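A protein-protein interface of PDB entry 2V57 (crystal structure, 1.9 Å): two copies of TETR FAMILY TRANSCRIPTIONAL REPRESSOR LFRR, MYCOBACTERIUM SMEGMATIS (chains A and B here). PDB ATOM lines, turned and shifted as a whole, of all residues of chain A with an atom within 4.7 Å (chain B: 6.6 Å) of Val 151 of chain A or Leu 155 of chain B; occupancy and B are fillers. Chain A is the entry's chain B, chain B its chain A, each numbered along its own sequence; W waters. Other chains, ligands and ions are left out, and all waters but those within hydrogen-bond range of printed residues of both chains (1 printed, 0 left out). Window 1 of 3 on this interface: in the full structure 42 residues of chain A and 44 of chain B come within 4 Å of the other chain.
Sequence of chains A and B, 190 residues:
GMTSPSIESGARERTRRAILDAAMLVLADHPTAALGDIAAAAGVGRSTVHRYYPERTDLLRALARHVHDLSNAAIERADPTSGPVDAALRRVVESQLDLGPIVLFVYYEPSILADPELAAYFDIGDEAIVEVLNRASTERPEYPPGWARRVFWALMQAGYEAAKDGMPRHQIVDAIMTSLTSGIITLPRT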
ATOM      1  N   TRP A 147       6.123  -1.630  26.561  1.00  0.00           N
ATOM      2  CA  TRP A 147       5.475  -0.467  25.928  1.00  0.00           C
ATOM      3  C   TRP A 147       4.115  -0.197  26.545  1.00  0.00           C
ATOM      4  O   TRP A 147       3.809   0.930  26.906  1.00  0.00           O
ATOM      5  CB  TRP A 147       5.309  -0.641  24.413  1.00  0.00           C
ATOM      6  CG  TRP A 147       4.784   0.629  23.738  1.00  0.00           C
ATOM      7  CD1 TRP A 147       3.565   0.810  23.137  1.00  0.00           C
ATOM      8  CD2 TRP A 147       5.467   1.887  23.651  1.00  0.00           C
ATOM      9  NE1 TRP A 147       3.458   2.104  22.658  1.00  0.00           N
ATOM     10  CE2 TRP A 147       4.609   2.784  22.964  1.00  0.00           C
ATOM     11  CE3 TRP A 147       6.722   2.341  24.086  1.00  0.00           C
ATOM     12  CZ2 TRP A 147       4.964   4.111  22.708  1.00  0.00           C
ATOM     13  CZ3 TRP A 147       7.078   3.664  23.822  1.00  0.00           C
ATOM     14  CH2 TRP A 147       6.199   4.531  23.144  1.00  0.00           C
ATOM     15  N   ALA A 148       3.291  -1.239  26.659  1.00  0.00           N
ATOM     16  CA  ALA A 148       1.944  -1.060  27.164  1.00  0.00           C
ATOM     17  C   ALA A 148       2.001  -0.556  28.591  1.00  0.00           C
ATOM     18  O   ALA A 148       1.239   0.325  28.967  1.00  0.00           O
ATOM     19  CB  ALA A 148       1.128  -2.359  27.069  1.00  0.00           C
ATOM     20  N   ARG A 149       2.889  -1.122  29.394  1.00  0.00           N
ATOM     21  CA  ARG A 149       2.984  -0.684  30.787  1.00  0.00           C
ATOM     22  C   ARG A 149       3.326   0.805  30.858  1.00  0.00           C
ATOM     23  O   ARG A 149       2.697   1.563  31.589  1.00  0.00           O
ATOM     24  CB  ARG A 149       4.026  -1.492  31.558  1.00  0.00           C
ATOM     25  CG  ARG A 149       4.124  -1.126  33.035  1.00  0.00           C
ATOM     26  CD  ARG A 149       4.854  -2.254  33.816  1.00  0.00           C
ATOM     27  NE  ARG A 149       6.293  -2.210  33.575  1.00  0.00           N
ATOM     28  CZ  ARG A 149       6.925  -2.947  32.668  1.00  0.00           C
ATOM     29  NH1 ARG A 149       6.244  -3.805  31.921  1.00  0.00           N
ATOM     30  NH2 ARG A 149       8.240  -2.820  32.508  1.00  0.00           N
ATOM     31  N   ARG A 150       4.343   1.207  30.114  1.00  0.00           N
ATOM     32  CA  ARG A 150       4.787   2.600  30.118  1.00  0.00           C
ATOM     33  C   ARG A 150       3.767   3.590  29.590  1.00  0.00           C
ATOM     34  O   ARG A 150       3.653   4.693  30.111  1.00  0.00           O
ATOM     35  CB  ARG A 150       6.080   2.745  29.341  1.00  0.00           C
ATOM     36  CG  ARG A 150       7.258   2.327  30.165  1.00  0.00           C
ATOM     37  CD  ARG A 150       8.322   1.702  29.327  1.00  0.00           C
ATOM     38  NE  ARG A 150       9.474   1.448  30.170  1.00  0.00           N
ATOM     39  CZ  ARG A 150      10.518   0.733  29.804  1.00  0.00           C
ATOM     40  NH1 ARG A 150      10.545   0.180  28.601  1.00  0.00           N
ATOM     41  NH2 ARG A 150      11.524   0.561  30.659  1.00  0.00           N
ATOM     42  N   VAL A 151       3.041   3.207  28.549  1.00  0.00           N
ATOM     43  CA  VAL A 151       1.987   4.052  28.030  1.00  0.00           C
ATOM     44  C   VAL A 151       0.856   4.172  29.056  1.00  0.00           C
ATOM     45  O   VAL A 151       0.347   5.249  29.276  1.00  0.00           O
ATOM     46  CB  VAL A 151       1.471   3.553  26.661  1.00  0.00           C
ATOM     47  CG1 VAL A 151       0.206   4.312  26.239  1.00  0.00           C
ATOM     48  CG2 VAL A 151       2.573   3.714  25.597  1.00  0.00           C
ATOM     49  N   PHE A 152       0.491   3.069  29.698  1.00  0.00           N
ATOM     50  CA  PHE A 152      -0.566   3.127  30.688  1.00  0.00           C
ATOM     51  C   PHE A 152      -0.226   4.147  31.754  1.00  0.00           C
ATOM     52  O   PHE A 152      -1.024   5.021  32.066  1.00  0.00           O
ATOM     53  CB  PHE A 152      -0.807   1.771  31.365  1.00  0.00           C
ATOM     54  CG  PHE A 152      -1.888   1.836  32.403  1.00  0.00           C
ATOM     55  CD1 PHE A 152      -3.226   1.656  32.053  1.00  0.00           C
ATOM     56  CD2 PHE A 152      -1.575   2.149  33.725  1.00  0.00           C
ATOM     57  CE1 PHE A 152      -4.222   1.742  33.021  1.00  0.00           C
ATOM     58  CE2 PHE A 152      -2.569   2.243  34.687  1.00  0.00           C
ATOM     59  CZ  PHE A 152      -3.892   2.028  34.332  1.00  0.00           C
ATOM     60  N   TRP A 153       0.980   4.063  32.292  1.00  0.00           N
ATOM     61  CA  TRP A 153       1.366   4.961  33.372  1.00  0.00           C
ATOM     62  C   TRP A 153       1.574   6.391  32.886  1.00  0.00           C
ATOM     63  O   TRP A 153       1.317   7.337  33.619  1.00  0.00           O
ATOM     64  CB  TRP A 153       2.593   4.407  34.112  1.00  0.00           C
ATOM     65  CG  TRP A 153       2.133   3.427  35.117  1.00  0.00           C
ATOM     66  CD1 TRP A 153       2.367   2.093  35.131  1.00  0.00           C
ATOM     67  CD2 TRP A 153       1.255   3.699  36.228  1.00  0.00           C
ATOM     68  NE1 TRP A 153       1.729   1.522  36.200  1.00  0.00           N
ATOM     69  CE2 TRP A 153       1.051   2.486  36.896  1.00  0.00           C
ATOM     70  CE3 TRP A 153       0.665   4.861  36.736  1.00  0.00           C
ATOM     71  CZ2 TRP A 153       0.252   2.385  38.049  1.00  0.00           C
ATOM     72  CZ3 TRP A 153      -0.124   4.769  37.877  1.00  0.00           C
ATOM     73  CH2 TRP A 153      -0.316   3.530  38.525  1.00  0.00           C
ATOM     74  N   ALA A 154       2.023   6.563  31.642  1.00  0.00           N
ATOM     75  CA  ALA A 154       2.159   7.920  31.125  1.00  0.00           C
ATOM     76  C   ALA A 154       0.789   8.585  30.980  1.00  0.00           C
ATOM     77  O   ALA A 154       0.619   9.766  31.305  1.00  0.00           O
ATOM     78  CB  ALA A 154       2.939   7.940  29.813  1.00  0.00           C
ATOM     79  N   LEU A 155      -0.192   7.815  30.511  1.00  0.00           N
ATOM     80  CA  LEU A 155      -1.528   8.331  30.356  1.00  0.00           C
ATOM     81  C   LEU A 155      -2.138   8.604  31.730  1.00  0.00           C
ATOM     82  O   LEU A 155      -2.857   9.574  31.894  1.00  0.00           O
ATOM     83  CB  LEU A 155      -2.419   7.377  29.554  1.00  0.00           C
ATOM     84  CG  LEU A 155      -2.179   7.215  28.052  1.00  0.00           C
ATOM     85  CD1 LEU A 155      -3.097   6.129  27.470  1.00  0.00           C
ATOM     86  CD2 LEU A 155      -2.417   8.520  27.338  1.00  0.00           C
ATOM     87  N   LEU B  97      13.284  12.679  20.664  1.00  0.00           N
ATOM     88  CA  LEU B  97      13.952  11.533  21.297  1.00  0.00           C
ATOM     89  C   LEU B  97      15.471  11.712  21.402  1.00  0.00           C
ATOM     90  O   LEU B  97      16.103  11.207  22.340  1.00  0.00           O
ATOM     91  CB  LEU B  97      13.652  10.213  20.573  1.00  0.00           C
ATOM     92  CG  LEU B  97      12.239   9.660  20.736  1.00  0.00           C
ATOM     93  CD1 LEU B  97      12.021   8.488  19.750  1.00  0.00           C
ATOM     94  CD2 LEU B  97      11.991   9.237  22.187  1.00  0.00           C
ATOM     95  N   ARG B 150      -1.617  16.503  25.796  1.00  0.00           N
ATOM     96  CA  ARG B 150      -1.143  15.675  26.904  1.00  0.00           C
ATOM     97  C   ARG B 150      -0.783  14.269  26.465  1.00  0.00           C
ATOM     98  O   ARG B 150       0.166  13.691  26.969  1.00  0.00           O
ATOM     99  CB  ARG B 150      -2.207  15.582  27.991  1.00  0.00           C
ATOM    100  CG  ARG B 150      -2.597  16.905  28.588  1.00  0.00           C
ATOM    101  CD  ARG B 150      -3.449  16.685  29.832  1.00  0.00           C
ATOM    102  NE  ARG B 150      -4.003  17.933  30.341  1.00  0.00           N
ATOM    103  CZ  ARG B 150      -3.362  18.792  31.131  1.00  0.00           C
ATOM    104  NH1 ARG B 150      -2.116  18.567  31.518  1.00  0.00           N
ATOM    105  NH2 ARG B 150      -3.985  19.890  31.537  1.00  0.00           N
ATOM    106  N   VAL B 151      -1.584  13.694  25.567  1.00  0.00           N
ATOM    107  CA  VAL B 151      -1.363  12.316  25.148  1.00  0.00           C
ATOM    108  C   VAL B 151      -0.083  12.223  24.326  1.00  0.00           C
ATOM    109  O   VAL B 151       0.682  11.274  24.465  1.00  0.00           O
ATOM    110  CB  VAL B 151      -2.551  11.798  24.319  1.00  0.00           C
ATOM    111  CG1 VAL B 151      -2.217  10.451  23.665  1.00  0.00           C
ATOM    112  CG2 VAL B 151      -3.801  11.706  25.181  1.00  0.00           C
ATOM    113  N   PHE B 152       0.154  13.217  23.474  1.00  0.00           N
ATOM    114  CA  PHE B 152       1.366  13.229  22.665  1.00  0.00           C
ATOM    115  C   PHE B 152       2.621  13.194  23.540  1.00  0.00           C
ATOM    116  O   PHE B 152       3.538  12.401  23.304  1.00  0.00           O
ATOM    117  CB  PHE B 152       1.399  14.484  21.727  1.00  0.00           C
ATOM    118  CG  PHE B 152       2.689  14.606  20.946  1.00  0.00           C
ATOM    119  CD1 PHE B 152       2.855  13.924  19.748  1.00  0.00           C
ATOM    120  CD2 PHE B 152       3.750  15.359  21.433  1.00  0.00           C
ATOM    121  CE1 PHE B 152       4.052  14.006  19.036  1.00  0.00           C
ATOM    122  CE2 PHE B 152       4.945  15.441  20.734  1.00  0.00           C
ATOM    123  CZ  PHE B 152       5.102  14.769  19.539  1.00  0.00           C
ATOM    124  N   TRP B 153       2.690  14.072  24.532  1.00  0.00           N
ATOM    125  CA  TRP B 153       3.870  14.125  25.390  1.00  0.00           C
ATOM    126  C   TRP B 153       3.932  12.929  26.349  1.00  0.00           C
ATOM    127  O   TRP B 153       5.013  12.551  26.803  1.00  0.00           O
ATOM    128  CB  TRP B 153       3.963  15.459  26.157  1.00  0.00           C
ATOM    129  CG  TRP B 153       4.249  16.619  25.236  1.00  0.00           C
ATOM    130  CD1 TRP B 153       3.407  17.645  24.919  1.00  0.00           C
ATOM    131  CD2 TRP B 153       5.447  16.839  24.477  1.00  0.00           C
ATOM    132  NE1 TRP B 153       4.006  18.494  24.022  1.00  0.00           N
ATOM    133  CE2 TRP B 153       5.264  18.028  23.741  1.00  0.00           C
ATOM    134  CE3 TRP B 153       6.659  16.153  24.358  1.00  0.00           C
ATOM    135  CZ2 TRP B 153       6.248  18.545  22.894  1.00  0.00           C
ATOM    136  CZ3 TRP B 153       7.640  16.675  23.528  1.00  0.00           C
ATOM    137  CH2 TRP B 153       7.429  17.855  22.805  1.00  0.00           C
ATOM    138  N   ALA B 154       2.780  12.331  26.629  1.00  0.00           N
ATOM    139  CA  ALA B 154       2.734  11.078  27.388  1.00  0.00           C
ATOM    140  C   ALA B 154       3.392   9.950  26.592  1.00  0.00           C
ATOM    141  O   ALA B 154       4.154   9.151  27.140  1.00  0.00           O
ATOM    142  CB  ALA B 154       1.310  10.717  27.760  1.00  0.00           C
ATOM    143  N   LEU B 155       3.090   9.879  25.302  1.00  0.00           N
ATOM    144  CA  LEU B 155       3.710   8.874  24.453  1.00  0.00           C
ATOM    145  C   LEU B 155       5.200   9.163  24.309  1.00  0.00           C
ATOM    146  O   LEU B 155       6.011   8.234  24.256  1.00  0.00           O
ATOM    147  CB  LEU B 155       3.016   8.783  23.096  1.00  0.00           C
ATOM    148  CG  LEU B 155       1.550   8.339  23.162  1.00  0.00           C
ATOM    149  CD1 LEU B 155       0.931   8.346  21.773  1.00  0.00           C
ATOM    150  CD2 LEU B 155       1.402   6.968  23.813  1.00  0.00           C
ATOM    151  N   MET B 156       5.569  10.446  24.235  1.00  0.00           N
ATOM    152  CA  MET B 156       6.989  10.824  24.231  1.00  0.00           C
ATOM    153  C   MET B 156       7.688  10.332  25.492  1.00  0.00           C
ATOM    154  O   MET B 156       8.808   9.813  25.432  1.00  0.00           O
ATOM    155  CB  MET B 156       7.168  12.333  24.084  1.00  0.00           C
ATOM    156  CG  MET B 156       6.928  12.828  22.647  1.00  0.00           C
ATOM    157  SD  MET B 156       8.085  12.109  21.472  1.00  0.00           S
ATOM    158  CE  MET B 156       9.609  12.213  22.356  1.00  0.00           C
ATOM    159  N   GLN B 157       7.036  10.505  26.638  1.00  0.00           N
ATOM    160  CA  GLN B 157       7.576   9.996  27.899  1.00  0.00           C
ATOM    161  C   GLN B 157       7.840   8.498  27.900  1.00  0.00           C
ATOM    162  O   GLN B 157       8.912   8.047  28.337  1.00  0.00           O
ATOM    163  CB  GLN B 157       6.652  10.317  29.077  1.00  0.00           C
ATOM    164  CG  GLN B 157       7.229   9.776  30.359  1.00  0.00           C
ATOM    165  CD  GLN B 157       6.327   9.967  31.554  1.00  0.00           C
ATOM    166  OE1 GLN B 157       5.876   9.002  32.175  1.00  0.00           O
ATOM    167  NE2 GLN B 157       6.067  11.208  31.885  1.00  0.00           N
ATOM    168  N   ALA B 158       6.880   7.716  27.420  1.00  0.00           N
ATOM    169  CA  ALA B 158       7.094   6.280  27.293  1.00  0.00           C
ATOM    170  C   ALA B 158       8.274   6.019  26.368  1.00  0.00           C
ATOM    171  O   ALA B 158       9.052   5.080  26.587  1.00  0.00           O
ATOM    172  CB  ALA B 158       5.838   5.593  26.766  1.00  0.00           C
ATOM    173  N   GLY B 159       8.399   6.843  25.323  1.00  0.00           N
ATOM    174  CA  GLY B 159       9.504   6.744  24.380  1.00  0.00           C
ATOM    175  C   GLY B 159      10.879   6.959  25.017  1.00  0.00           C
ATOM    176  O   GLY B 159      11.823   6.210  24.775  1.00  0.00           O
ATOM    177  N   TYR B 160      10.999   7.989  25.843  1.00  0.00           N
ATOM    178  CA  TYR B 160      12.250   8.225  26.547  1.00  0.00           C
ATOM    179  C   TYR B 160      12.605   7.049  27.439  1.00  0.00           C
ATOM    180  O   TYR B 160      13.771   6.668  27.534  1.00  0.00           O
ATOM    181  CB  TYR B 160      12.171   9.493  27.389  1.00  0.00           C
ATOM    182  CG  TYR B 160      12.198  10.773  26.578  1.00  0.00           C
ATOM    183  CD1 TYR B 160      13.329  11.127  25.827  1.00  0.00           C
ATOM    184  CD2 TYR B 160      11.104  11.635  26.578  1.00  0.00           C
ATOM    185  CE1 TYR B 160      13.355  12.320  25.078  1.00  0.00           C
ATOM    186  CE2 TYR B 160      11.121  12.820  25.828  1.00  0.00           C
ATOM    187  CZ  TYR B 160      12.247  13.151  25.094  1.00  0.00           C
ATOM    188  OH  TYR B 160      12.273  14.319  24.370  1.00  0.00           O
ATOM    189  N   ILE B 172      10.934   2.773  18.555  1.00  0.00           N
ATOM    190  CA  ILE B 172      10.223   3.707  19.414  1.00  0.00           C
ATOM    191  C   ILE B 172       9.314   4.618  18.589  1.00  0.00           C
ATOM    192  O   ILE B 172       8.151   4.851  18.938  1.00  0.00           O
ATOM    193  CB  ILE B 172      11.197   4.571  20.244  1.00  0.00           C
ATOM    194  CG1 ILE B 172      12.146   3.682  21.052  1.00  0.00           C
ATOM    195  CG2 ILE B 172      10.410   5.503  21.177  1.00  0.00           C
ATOM    196  CD1 ILE B 172      13.206   4.466  21.809  1.00  0.00           C
ATOM    197  N   ALA B 175       6.345   2.769  17.433  1.00  0.00           N
ATOM    198  CA  ALA B 175       5.424   2.512  18.546  1.00  0.00           C
ATOM    199  C   ALA B 175       4.620   3.773  18.899  1.00  0.00           C
ATOM    200  O   ALA B 175       3.429   3.709  19.235  1.00  0.00           O
ATOM    201  CB  ALA B 175       6.175   2.004  19.759  1.00  0.00           C
ATOM    202  N   ILE B 176       5.284   4.920  18.854  1.00  0.00           N
ATOM    203  CA  ILE B 176       4.604   6.166  19.167  1.00  0.00           C
ATOM    204  C   ILE B 176       3.577   6.488  18.093  1.00  0.00           C
ATOM    205  O   ILE B 176       2.439   6.833  18.400  1.00  0.00           O
ATOM    206  CB  ILE B 176       5.622   7.328  19.337  1.00  0.00           C
ATOM    207  CG1 ILE B 176       6.352   7.155  20.678  1.00  0.00           C
ATOM    208  CG2 ILE B 176       4.917   8.699  19.244  1.00  0.00           C
ATOM    209  CD1 ILE B 176       7.498   8.109  20.921  1.00  0.00           C
ATOM    210  N   MET B 177       3.967   6.345  16.832  1.00  0.00           N
ATOM    211  CA  MET B 177       3.057   6.683  15.734  1.00  0.00           C
ATOM    212  C   MET B 177       1.832   5.757  15.743  1.00  0.00           C
ATOM    213  O   MET B 177       0.700   6.199  15.565  1.00  0.00           O
ATOM    214  CB  MET B 177       3.785   6.631  14.379  1.00  0.00           C
ATOM    215  CG  MET B 177       4.888   7.680  14.248  1.00  0.00           C
ATOM    216  SD  MET B 177       4.294   9.381  14.454  1.00  0.00           S
ATOM    217  CE  MET B 177       3.002   9.395  13.195  1.00  0.00           C
ATOM    218  N   THR B 178       2.059   4.475  15.979  1.00  0.00           N
ATOM    219  CA  THR B 178       0.941   3.542  16.080  1.00  0.00           C
ATOM    220  C   THR B 178       0.048   3.864  17.271  1.00  0.00           C
ATOM    221  O   THR B 178      -1.195   3.784  17.183  1.00  0.00           O
ATOM    222  CB  THR B 178       1.440   2.093  16.151  1.00  0.00           C
ATOM    223  OG1 THR B 178       2.140   1.789  14.938  1.00  0.00           O
ATOM    224  CG2 THR B 178       0.275   1.137  16.292  1.00  0.00           C
ATOM    225  N   SER B 179       0.658   4.257  18.388  1.00  0.00           N
ATOM    226  CA  SER B 179      -0.138   4.561  19.575  1.00  0.00           C
ATOM    227  C   SER B 179      -0.999   5.822  19.355  1.00  0.00           C
ATOM    228  O   SER B 179      -2.145   5.882  19.801  1.00  0.00           O
ATOM    229  CB  SER B 179       0.752   4.707  20.815  1.00  0.00           C
ATOM    230  OG  SER B 179       1.379   3.471  21.137  1.00  0.00           O
ATOM    231  N   LEU B 180      -0.443   6.807  18.654  1.00  0.00           N
ATOM    232  CA  LEU B 180      -1.169   8.029  18.316  1.00  0.00           C
ATOM    233  C   LEU B 180      -2.422   7.767  17.467  1.00  0.00           C
ATOM    234  O   LEU B 180      -3.457   8.418  17.642  1.00  0.00           O
ATOM    235  CB  LEU B 180      -0.250   8.984  17.563  1.00  0.00           C
ATOM    236  CG  LEU B 180       0.754   9.755  18.416  1.00  0.00           C
ATOM    237  CD1 LEU B 180       1.805  10.438  17.554  1.00  0.00           C
ATOM    238  CD2 LEU B 180       0.003  10.741  19.258  1.00  0.00           C
ATOM    239  N   THR B 181      -2.317   6.819  16.544  1.00  0.00           N
ATOM    240  CA  THR B 181      -3.399   6.557  15.602  1.00  0.00           C
ATOM    241  C   THR B 181      -4.365   5.458  16.047  1.00  0.00           C
ATOM    242  O   THR B 181      -5.524   5.444  15.617  1.00  0.00           O
ATOM    243  CB  THR B 181      -2.846   6.218  14.184  1.00  0.00           C
ATOM    244  OG1 THR B 181      -2.016   5.049  14.246  1.00  0.00           O
ATOM    245  CG2 THR B 181      -2.028   7.374  13.632  1.00  0.00           C
ATOM    246  N   GLY B 183      -4.045   3.722  19.584  1.00  0.00           N
ATOM    247  CA  GLY B 183      -4.021   3.379  20.996  1.00  0.00           C
ATOM    248  C   GLY B 183      -3.190   2.114  21.189  1.00  0.00           C
ATOM    249  O   GLY B 183      -2.454   1.711  20.286  1.00  0.00           O
ATOM    250  N   ILE B 184      -3.279   1.483  22.353  1.00  0.00           N
ATOM    251  CA  ILE B 184      -2.453   0.305  22.582  1.00  0.00           C
ATOM    252  C   ILE B 184      -3.225  -0.992  22.682  1.00  0.00           C
ATOM    253  O   ILE B 184      -2.610  -2.047  22.694  1.00  0.00           O
ATOM    254  CB  ILE B 184      -1.529   0.437  23.812  1.00  0.00           C
ATOM    255  CG1 ILE B 184      -2.312   0.862  25.046  1.00  0.00           C
ATOM    256  CG2 ILE B 184      -0.414   1.427  23.532  1.00  0.00           C
ATOM    257  CD1 ILE B 184      -1.561   0.581  26.366  1.00  0.00           C
HETATM  258  O   HOH W   1       5.418   6.070  31.477  1.00  0.00           O
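NE1 of Trp 147 of chain A is in hydrogen-bond range of OG of Ser 179 of chain B (2.9 Å).
The side-chain hydroxyl (OG) of Ser 179 of chain B sits at hydrogen-bond distance from the backbone carbonyl oxygen (O) of Ala 175 of chain B (2.8 Å).
Trp 147 of chain A touches Leu 155 of chain B (CH2 to O, 3.9 Å). Trp 147 of chain A touches Ala 158 of chain B. Trp 147 of chain A touches Gly 159 of chain B (CZ3 to N, 3.8 Å). Ile 176 of chain B touches Trp 147 of chain A. Ile 184 of chain B touches Ala 148 of chain A (CD1 to O, 3.8 Å). Ala 158 of chain B touches Arg 150 of chain A (CB to CB, 3.8 Å). Val 151 of chain A touches Leu 155 of chain B. CB of Ala 158 of chain B touches CG2 of Val 151 of chain A (3.9 Å). Ala 154 of chain A touches Ala 154 of chain B. OE1 of Gln 157 of chain B touches CB of Ala 154 of chain A (3.9 Å).
Of the printed residues of chain B, Val 151 of chain A touches Leu 155 (3.8 Å) and Ala 158 (3.9 Å). Leu 155 of chain B touches two residues of chain A. Of the printed residues of chain A, Ala 175 of chain B touches Trp 147. Of the printed residues of chain B, Ala 148 of chain A touches Ile 184 (3.8 Å). Of the printed residues of chain A, Ala 154 of chain B touches Ala 154 (3.2 Å). Of the printed residues of chain B, Arg 150 of chain A touches Ala 158. Tyr 160 of chain B touches none of the printed residues of chain A. Thr 178 of chain B touches none of the printed residues of chain A. The nearest printed residue of chain B that does not touch Val 151 of chain A is Ile 184 of chain B (4.004 Å). The nearest printed residue of chain A that does not touch Leu 155 of chain B is Ala 154 of chain A (4.9 Å). The nearest printed residue of chain A that does not touch Gly 159 of chain B is Arg 150 of chain A (6.2 Å).
Of the 22 printed residues of chain B, 9 touch a printed residue of chain A. Hydrophobic or aromatic side chains of chain B that line the printed part of chain A: Ala 154, Leu 155, Ala 158, Ala 175, Ile 176 and Ile 184.
Val 151 of chain A touches Leu 155 of chain B, but with the chains exchanged Leu 155 of chain A does not touch Val 151 of chain B (4.1 Å). Ala 154 of chain B touches its own counterpart, Ala 154 of chain A. Positions printed for both chains: 150, 151, 152, 153, 154 and 155. Of the 12 pairs that touch across the chains among the printed residues, 1 has its exchanged pair printed and touching as well.
Water W1 lies within hydrogen-bond range of the backbone carbonyl oxygen (O) of Arg 150 of chain A (2.6 Å), the side-chain amide oxygen (OE1) of Gln 157 of chain B (3.0 Å) and the backbone NH (N) of Ala 154 of chain A (3.4 Å).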
